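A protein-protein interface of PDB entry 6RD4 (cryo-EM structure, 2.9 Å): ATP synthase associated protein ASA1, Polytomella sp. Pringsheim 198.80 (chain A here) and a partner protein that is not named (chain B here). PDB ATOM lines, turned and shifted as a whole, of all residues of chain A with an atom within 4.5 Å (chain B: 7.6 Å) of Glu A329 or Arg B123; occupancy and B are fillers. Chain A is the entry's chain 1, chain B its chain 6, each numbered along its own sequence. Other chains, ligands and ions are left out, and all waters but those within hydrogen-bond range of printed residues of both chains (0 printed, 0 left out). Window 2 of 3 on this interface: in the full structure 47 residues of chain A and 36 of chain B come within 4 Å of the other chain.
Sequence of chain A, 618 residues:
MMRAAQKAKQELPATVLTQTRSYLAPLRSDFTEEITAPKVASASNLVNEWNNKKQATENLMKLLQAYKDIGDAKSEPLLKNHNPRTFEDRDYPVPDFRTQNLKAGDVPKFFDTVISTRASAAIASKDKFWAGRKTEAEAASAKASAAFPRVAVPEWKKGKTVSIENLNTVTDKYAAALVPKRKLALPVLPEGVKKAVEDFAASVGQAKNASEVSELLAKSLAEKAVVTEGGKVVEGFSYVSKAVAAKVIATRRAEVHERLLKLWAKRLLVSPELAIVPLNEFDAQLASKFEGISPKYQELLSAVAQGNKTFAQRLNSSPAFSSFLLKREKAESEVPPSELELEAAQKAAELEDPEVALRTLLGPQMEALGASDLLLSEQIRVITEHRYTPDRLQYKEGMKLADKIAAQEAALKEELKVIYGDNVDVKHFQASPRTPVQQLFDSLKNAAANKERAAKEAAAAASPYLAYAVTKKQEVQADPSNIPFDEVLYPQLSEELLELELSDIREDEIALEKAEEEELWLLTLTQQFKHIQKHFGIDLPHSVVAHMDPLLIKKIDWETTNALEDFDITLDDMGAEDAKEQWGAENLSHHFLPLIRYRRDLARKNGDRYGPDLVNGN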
ATOM      1  N   ASN A 316       3.319 -12.895   8.161  1.00  0.00           N
ATOM      2  CA  ASN A 316       3.295 -12.257   9.466  1.00  0.00           C
ATOM      3  C   ASN A 316       3.103 -10.765   9.356  1.00  0.00           C
ATOM      4  O   ASN A 316       2.570 -10.140  10.274  1.00  0.00           O
ATOM      5  CB  ASN A 316       4.584 -12.541  10.194  1.00  0.00           C
ATOM      6  CG  ASN A 316       4.559 -13.835  10.872  1.00  0.00           C
ATOM      7  OD1 ASN A 316       5.505 -14.600  10.818  1.00  0.00           O
ATOM      8  ND2 ASN A 316       3.469 -14.104  11.539  1.00  0.00           N
ATOM      9  N   PHE A 321      -2.572 -10.602  10.191  1.00  0.00           N
ATOM     10  CA  PHE A 321      -1.916 -10.922  11.442  1.00  0.00           C
ATOM     11  C   PHE A 321      -1.732  -9.704  12.317  1.00  0.00           C
ATOM     12  O   PHE A 321      -1.254  -9.826  13.438  1.00  0.00           O
ATOM     13  CB  PHE A 321      -0.588 -11.605  11.168  1.00  0.00           C
ATOM     14  CG  PHE A 321      -0.725 -13.059  10.925  1.00  0.00           C
ATOM     15  CD1 PHE A 321      -0.424 -13.966  11.900  1.00  0.00           C
ATOM     16  CD2 PHE A 321      -1.205 -13.516   9.736  1.00  0.00           C
ATOM     17  CE1 PHE A 321      -0.588 -15.295  11.678  1.00  0.00           C
ATOM     18  CE2 PHE A 321      -1.356 -14.834   9.515  1.00  0.00           C
ATOM     19  CZ  PHE A 321      -1.053 -15.724  10.491  1.00  0.00           C
ATOM     20  N   LEU A 326      -5.451 -12.398  15.777  1.00  0.00           N
ATOM     21  CA  LEU A 326      -4.235 -13.011  15.274  1.00  0.00           C
ATOM     22  C   LEU A 326      -3.012 -12.188  15.610  1.00  0.00           C
ATOM     23  O   LEU A 326      -1.969 -12.375  14.995  1.00  0.00           O
ATOM     24  CB  LEU A 326      -4.313 -13.207  13.765  1.00  0.00           C
ATOM     25  CG  LEU A 326      -5.223 -14.284  13.219  1.00  0.00           C
ATOM     26  CD1 LEU A 326      -5.101 -14.274  11.756  1.00  0.00           C
ATOM     27  CD2 LEU A 326      -4.784 -15.590  13.753  1.00  0.00           C
ATOM     28  N   LYS A 327      -3.118 -11.293  16.589  1.00  0.00           N
ATOM     29  CA  LYS A 327      -2.070 -10.306  16.812  1.00  0.00           C
ATOM     30  C   LYS A 327      -0.840 -10.922  17.459  1.00  0.00           C
ATOM     31  O   LYS A 327       0.289 -10.578  17.104  1.00  0.00           O
ATOM     32  CB  LYS A 327      -2.604  -9.170  17.664  1.00  0.00           C
ATOM     33  CG  LYS A 327      -1.910  -7.888  17.415  1.00  0.00           C
ATOM     34  CD  LYS A 327      -2.606  -6.751  18.096  1.00  0.00           C
ATOM     35  CE  LYS A 327      -3.880  -6.420  17.404  1.00  0.00           C
ATOM     36  NZ  LYS A 327      -4.538  -5.240  17.987  1.00  0.00           N
ATOM     37  N   ARG A 328      -1.071 -11.850  18.393  1.00  0.00           N
ATOM     38  CA  ARG A 328       0.039 -12.531  19.112  1.00  0.00           C
ATOM     39  C   ARG A 328       0.329 -13.885  18.455  1.00  0.00           C
ATOM     40  O   ARG A 328       0.884 -14.763  19.142  1.00  0.00           O
ATOM     41  CB  ARG A 328      -0.313 -12.703  20.594  1.00  0.00           C
ATOM     42  CG  ARG A 328      -0.428 -11.394  21.361  1.00  0.00           C
ATOM     43  CD  ARG A 328      -0.706 -11.612  22.839  1.00  0.00           C
ATOM     44  NE  ARG A 328      -0.839 -10.358  23.566  1.00  0.00           N
ATOM     45  CZ  ARG A 328       0.182  -9.646  24.031  1.00  0.00           C
ATOM     46  NH1 ARG A 328       1.422 -10.064  23.841  1.00  0.00           N
ATOM     47  NH2 ARG A 328      -0.041  -8.519  24.682  1.00  0.00           N
ATOM     48  N   GLU A 329      -0.033 -14.044  17.176  1.00  0.00           N
ATOM     49  CA  GLU A 329       0.214 -15.293  16.482  1.00  0.00           C
ATOM     50  C   GLU A 329       1.344 -15.142  15.481  1.00  0.00           C
ATOM     51  O   GLU A 329       1.675 -14.043  15.036  1.00  0.00           O
ATOM     52  CB  GLU A 329      -1.040 -15.774  15.764  1.00  0.00           C
ATOM     53  CG  GLU A 329      -2.038 -16.423  16.662  1.00  0.00           C
ATOM     54  CD  GLU A 329      -1.425 -17.491  17.517  1.00  0.00           C
ATOM     55  OE1 GLU A 329      -1.616 -17.438  18.747  1.00  0.00           O
ATOM     56  OE2 GLU A 329      -0.745 -18.385  16.972  1.00  0.00           O
ATOM     57  N   LYS A 330       1.929 -16.270  15.128  1.00  0.00           N
ATOM     58  CA  LYS A 330       2.992 -16.309  14.149  1.00  0.00           C
ATOM     59  C   LYS A 330       2.644 -17.345  13.099  1.00  0.00           C
ATOM     60  O   LYS A 330       2.155 -18.424  13.424  1.00  0.00           O
ATOM     61  CB  LYS A 330       4.327 -16.630  14.808  1.00  0.00           C
ATOM     62  CG  LYS A 330       4.870 -15.495  15.647  1.00  0.00           C
ATOM     63  CD  LYS A 330       4.995 -14.238  14.820  1.00  0.00           C
ATOM     64  CE  LYS A 330       4.922 -12.997  15.673  1.00  0.00           C
ATOM     65  NZ  LYS A 330       4.954 -11.777  14.819  1.00  0.00           N
ATOM     66  N   ALA A 331       2.893 -17.008  11.839  1.00  0.00           N
ATOM     67  CA  ALA A 331       2.563 -17.897  10.741  1.00  0.00           C
ATOM     68  C   ALA A 331       3.485 -19.095  10.672  1.00  0.00           C
ATOM     69  O   ALA A 331       3.112 -20.112  10.087  1.00  0.00           O
ATOM     70  CB  ALA A 331       2.618 -17.139   9.427  1.00  0.00           C
ATOM     71  N   SER A 333       4.234 -20.863  13.156  1.00  0.00           N
ATOM     72  CA  SER A 333       3.709 -21.832  14.100  1.00  0.00           C
ATOM     73  C   SER A 333       2.792 -22.838  13.438  1.00  0.00           C
ATOM     74  O   SER A 333       2.527 -23.891  14.022  1.00  0.00           O
ATOM     75  CB  SER A 333       2.963 -21.112  15.213  1.00  0.00           C
ATOM     76  OG  SER A 333       3.837 -20.255  15.915  1.00  0.00           O
ATOM     77  N   GLU A 334       2.278 -22.538  12.250  1.00  0.00           N
ATOM     78  CA  GLU A 334       1.389 -23.481  11.592  1.00  0.00           C
ATOM     79  C   GLU A 334       2.172 -24.465  10.743  1.00  0.00           C
ATOM     80  O   GLU A 334       2.185 -25.666  11.025  1.00  0.00           O
ATOM     81  CB  GLU A 334       0.361 -22.742  10.744  1.00  0.00           C
ATOM     82  CG  GLU A 334      -0.604 -23.669  10.039  1.00  0.00           C
ATOM     83  CD  GLU A 334      -1.786 -24.069  10.901  1.00  0.00           C
ATOM     84  OE1 GLU A 334      -1.840 -23.655  12.075  1.00  0.00           O
ATOM     85  OE2 GLU A 334      -2.669 -24.791  10.395  1.00  0.00           O
ATOM     86  N   ILE B 120     -11.587 -21.096  20.732  1.00  0.00           N
ATOM     87  CA  ILE B 120     -11.386 -21.306  19.301  1.00  0.00           C
ATOM     88  C   ILE B 120      -9.916 -21.086  18.977  1.00  0.00           C
ATOM     89  O   ILE B 120      -9.357 -20.048  19.358  1.00  0.00           O
ATOM     90  CB  ILE B 120     -12.268 -20.366  18.498  1.00  0.00           C
ATOM     91  CG1 ILE B 120     -13.730 -20.699  18.717  1.00  0.00           C
ATOM     92  CG2 ILE B 120     -11.978 -20.507  17.040  1.00  0.00           C
ATOM     93  CD1 ILE B 120     -14.660 -19.748  18.041  1.00  0.00           C
ATOM     94  N   PRO B 121      -9.241 -22.026  18.341  1.00  0.00           N
ATOM     95  CA  PRO B 121      -7.868 -21.760  17.917  1.00  0.00           C
ATOM     96  C   PRO B 121      -7.861 -20.854  16.707  1.00  0.00           C
ATOM     97  O   PRO B 121      -8.066 -21.305  15.584  1.00  0.00           O
ATOM     98  CB  PRO B 121      -7.327 -23.151  17.603  1.00  0.00           C
ATOM     99  CG  PRO B 121      -8.516 -23.973  17.311  1.00  0.00           C
ATOM    100  CD  PRO B 121      -9.670 -23.397  18.031  1.00  0.00           C
ATOM    101  N   PHE B 122      -7.596 -19.572  16.911  1.00  0.00           N
ATOM    102  CA  PHE B 122      -7.835 -18.614  15.850  1.00  0.00           C
ATOM    103  C   PHE B 122      -6.760 -18.622  14.787  1.00  0.00           C
ATOM    104  O   PHE B 122      -6.996 -18.121  13.693  1.00  0.00           O
ATOM    105  CB  PHE B 122      -7.963 -17.223  16.428  1.00  0.00           C
ATOM    106  CG  PHE B 122      -9.254 -16.980  17.093  1.00  0.00           C
ATOM    107  CD1 PHE B 122     -10.404 -16.866  16.356  1.00  0.00           C
ATOM    108  CD2 PHE B 122      -9.325 -16.856  18.456  1.00  0.00           C
ATOM    109  CE1 PHE B 122     -11.596 -16.631  16.965  1.00  0.00           C
ATOM    110  CE2 PHE B 122     -10.513 -16.616  19.066  1.00  0.00           C
ATOM    111  CZ  PHE B 122     -11.649 -16.505  18.319  1.00  0.00           C
ATOM    112  N   ARG B 123      -5.588 -19.154  15.081  1.00  0.00           N
ATOM    113  CA  ARG B 123      -4.597 -19.321  14.039  1.00  0.00           C
ATOM    114  C   ARG B 123      -4.831 -20.595  13.270  1.00  0.00           C
ATOM    115  O   ARG B 123      -4.523 -20.663  12.085  1.00  0.00           O
ATOM    116  CB  ARG B 123      -3.202 -19.318  14.631  1.00  0.00           C
ATOM    117  CG  ARG B 123      -2.108 -19.085  13.636  1.00  0.00           C
ATOM    118  CD  ARG B 123      -0.901 -19.895  13.984  1.00  0.00           C
ATOM    119  NE  ARG B 123      -1.242 -21.293  14.178  1.00  0.00           N
ATOM    120  CZ  ARG B 123      -1.008 -21.962  15.296  1.00  0.00           C
ATOM    121  NH1 ARG B 123      -0.438 -21.355  16.318  1.00  0.00           N
ATOM    122  NH2 ARG B 123      -1.351 -23.233  15.394  1.00  0.00           N
ATOM    123  N   ALA B 124      -5.365 -21.613  13.916  1.00  0.00           N
ATOM    124  CA  ALA B 124      -5.689 -22.828  13.200  1.00  0.00           C
ATOM    125  C   ALA B 124      -6.932 -22.658  12.364  1.00  0.00           C
ATOM    126  O   ALA B 124      -7.054 -23.298  11.324  1.00  0.00           O
ATOM    127  CB  ALA B 124      -5.875 -23.978  14.171  1.00  0.00           C
ATOM    128  N   VAL B 125      -7.858 -21.810  12.800  1.00  0.00           N
ATOM    129  CA  VAL B 125      -9.058 -21.512  12.029  1.00  0.00           C
ATOM    130  C   VAL B 125      -8.718 -20.662  10.817  1.00  0.00           C
ATOM    131  O   VAL B 125      -9.279 -20.858   9.738  1.00  0.00           O
ATOM    132  CB  VAL B 125     -10.093 -20.845  12.950  1.00  0.00           C
ATOM    133  CG1 VAL B 125     -11.140 -20.111  12.202  1.00  0.00           C
ATOM    134  CG2 VAL B 125     -10.756 -21.891  13.768  1.00  0.00           C
ATOM    135  N   TYR B 126      -7.769 -19.738  10.962  1.00  0.00           N
ATOM    136  CA  TYR B 126      -7.347 -18.900   9.848  1.00  0.00           C
ATOM    137  C   TYR B 126      -6.694 -19.727   8.760  1.00  0.00           C
ATOM    138  O   TYR B 126      -6.936 -19.508   7.575  1.00  0.00           O
ATOM    139  CB  TYR B 126      -6.381 -17.830  10.333  1.00  0.00           C
ATOM    140  CG  TYR B 126      -5.816 -16.989   9.231  1.00  0.00           C
ATOM    141  CD1 TYR B 126      -6.561 -15.986   8.664  1.00  0.00           C
ATOM    142  CD2 TYR B 126      -4.538 -17.192   8.759  1.00  0.00           C
ATOM    143  CE1 TYR B 126      -6.062 -15.231   7.659  1.00  0.00           C
ATOM    144  CE2 TYR B 126      -4.040 -16.446   7.751  1.00  0.00           C
ATOM    145  CZ  TYR B 126      -4.806 -15.466   7.210  1.00  0.00           C
ATOM    146  OH  TYR B 126      -4.307 -14.707   6.202  1.00  0.00           O
ATOM    147  N   PHE B 127      -5.863 -20.677   9.135  1.00  0.00           N
ATOM    148  CA  PHE B 127      -5.206 -21.505   8.145  1.00  0.00           C
ATOM    149  C   PHE B 127      -6.082 -22.637   7.670  1.00  0.00           C
ATOM    150  O   PHE B 127      -5.730 -23.297   6.694  1.00  0.00           O
ATOM    151  CB  PHE B 127      -3.907 -22.061   8.706  1.00  0.00           C
ATOM    152  CG  PHE B 127      -2.778 -21.103   8.640  1.00  0.00           C
ATOM    153  CD1 PHE B 127      -2.088 -20.926   7.474  1.00  0.00           C
ATOM    154  CD2 PHE B 127      -2.417 -20.366   9.737  1.00  0.00           C
ATOM    155  CE1 PHE B 127      -1.066 -20.033   7.411  1.00  0.00           C
ATOM    156  CE2 PHE B 127      -1.398 -19.481   9.672  1.00  0.00           C
ATOM    157  CZ  PHE B 127      -0.724 -19.316   8.513  1.00  0.00           C
ATOM    158  N   ALA B 128      -7.200 -22.887   8.329  1.00  0.00           N
ATOM    159  CA  ALA B 128      -8.174 -23.837   7.829  1.00  0.00           C
ATOM    160  C   ALA B 128      -9.108 -23.220   6.820  1.00  0.00           C
ATOM    161  O   ALA B 128      -9.644 -23.936   5.983  1.00  0.00           O
ATOM    162  CB  ALA B 128      -9.004 -24.413   8.965  1.00  0.00           C
ATOM    163  N   PHE B 129      -9.348 -21.919   6.901  1.00  0.00           N
ATOM    164  CA  PHE B 129     -10.130 -21.266   5.862  1.00  0.00           C
ATOM    165  C   PHE B 129      -9.280 -21.003   4.643  1.00  0.00           C
ATOM    166  O   PHE B 129      -9.802 -20.946   3.535  1.00  0.00           O
ATOM    167  CB  PHE B 129     -10.732 -19.961   6.362  1.00  0.00           C
ATOM    168  CG  PHE B 129     -11.864 -20.139   7.331  1.00  0.00           C
ATOM    169  CD1 PHE B 129     -12.425 -21.367   7.567  1.00  0.00           C
ATOM    170  CD2 PHE B 129     -12.363 -19.067   8.007  1.00  0.00           C
ATOM    171  CE1 PHE B 129     -13.439 -21.509   8.448  1.00  0.00           C
ATOM    172  CE2 PHE B 129     -13.385 -19.211   8.880  1.00  0.00           C
ATOM    173  CZ  PHE B 129     -13.918 -20.430   9.100  1.00  0.00           C
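Tyr B126 touches Phe A321.
Phe A321 touches Phe B127 (CZ to CE2, 3.9 Å).
Phe B122 touches Leu A326 (O to CD2, 3.4 Å).
CD2 of Leu A326 touches CA of Arg B123 (3.7 Å).
CG of Tyr B126 touches CD1 of Leu A326, at 3.8 Å.
Arg B123 touches Lys A330.
Arg B123 touches Ser A333 (NH1 to CB, 3.6 Å).
Glu A334 touches Phe B127 (OE2 to CB, 3.4 Å).
OE2 of Glu A329 is in salt-bridge range of NH1 of Arg B123, at 3.1 Å.
NE of Arg B123 lies within salt-bridge range of OE1 of Glu A334 (3.2 Å).
Glu A329 touches just one residue of chain B: Arg B123.
Arg B123 touches just these residues of chain A: Leu A326, Glu A329, Lys A330, Ser A333 and Glu A334.
Of the printed residues of chain B, Phe A321 touches Tyr B126 (3.6 Å) and Phe B127 (3.9 Å).
Printed residues of chain A within 4 Å of Phe B122: Leu A326 (3.4 Å).
Printed residues of chain B within 4 Å of Leu A326: Phe B122 (3.4 Å), Arg B123 (3.7 Å) and Tyr B126 (3.8 Å).
Ala B128 touches none of the printed residues of chain A.
Ile B120 touches none of the printed residues of chain A.
Hydrophobic or aromatic side chains of chain B that line the printed part of chain A: Tyr B126 and Phe B127.
Along chain B the printed residues that touch a printed residue of chain A span positions 122 to 127.
Hydrophobic or aromatic side chains of chain A that line the printed part of chain B: Phe A321 and Leu A326.
Among the printed residues, 10 pairs touch across the chains.
Among the printed residues, Asp or Glu carboxylates within 4 Å of a Lys or Arg side-chain nitrogen of the other chain: Glu A329 with Arg B123 (3.1 Å) and Glu A334 with Arg B123 (3.2 Å).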
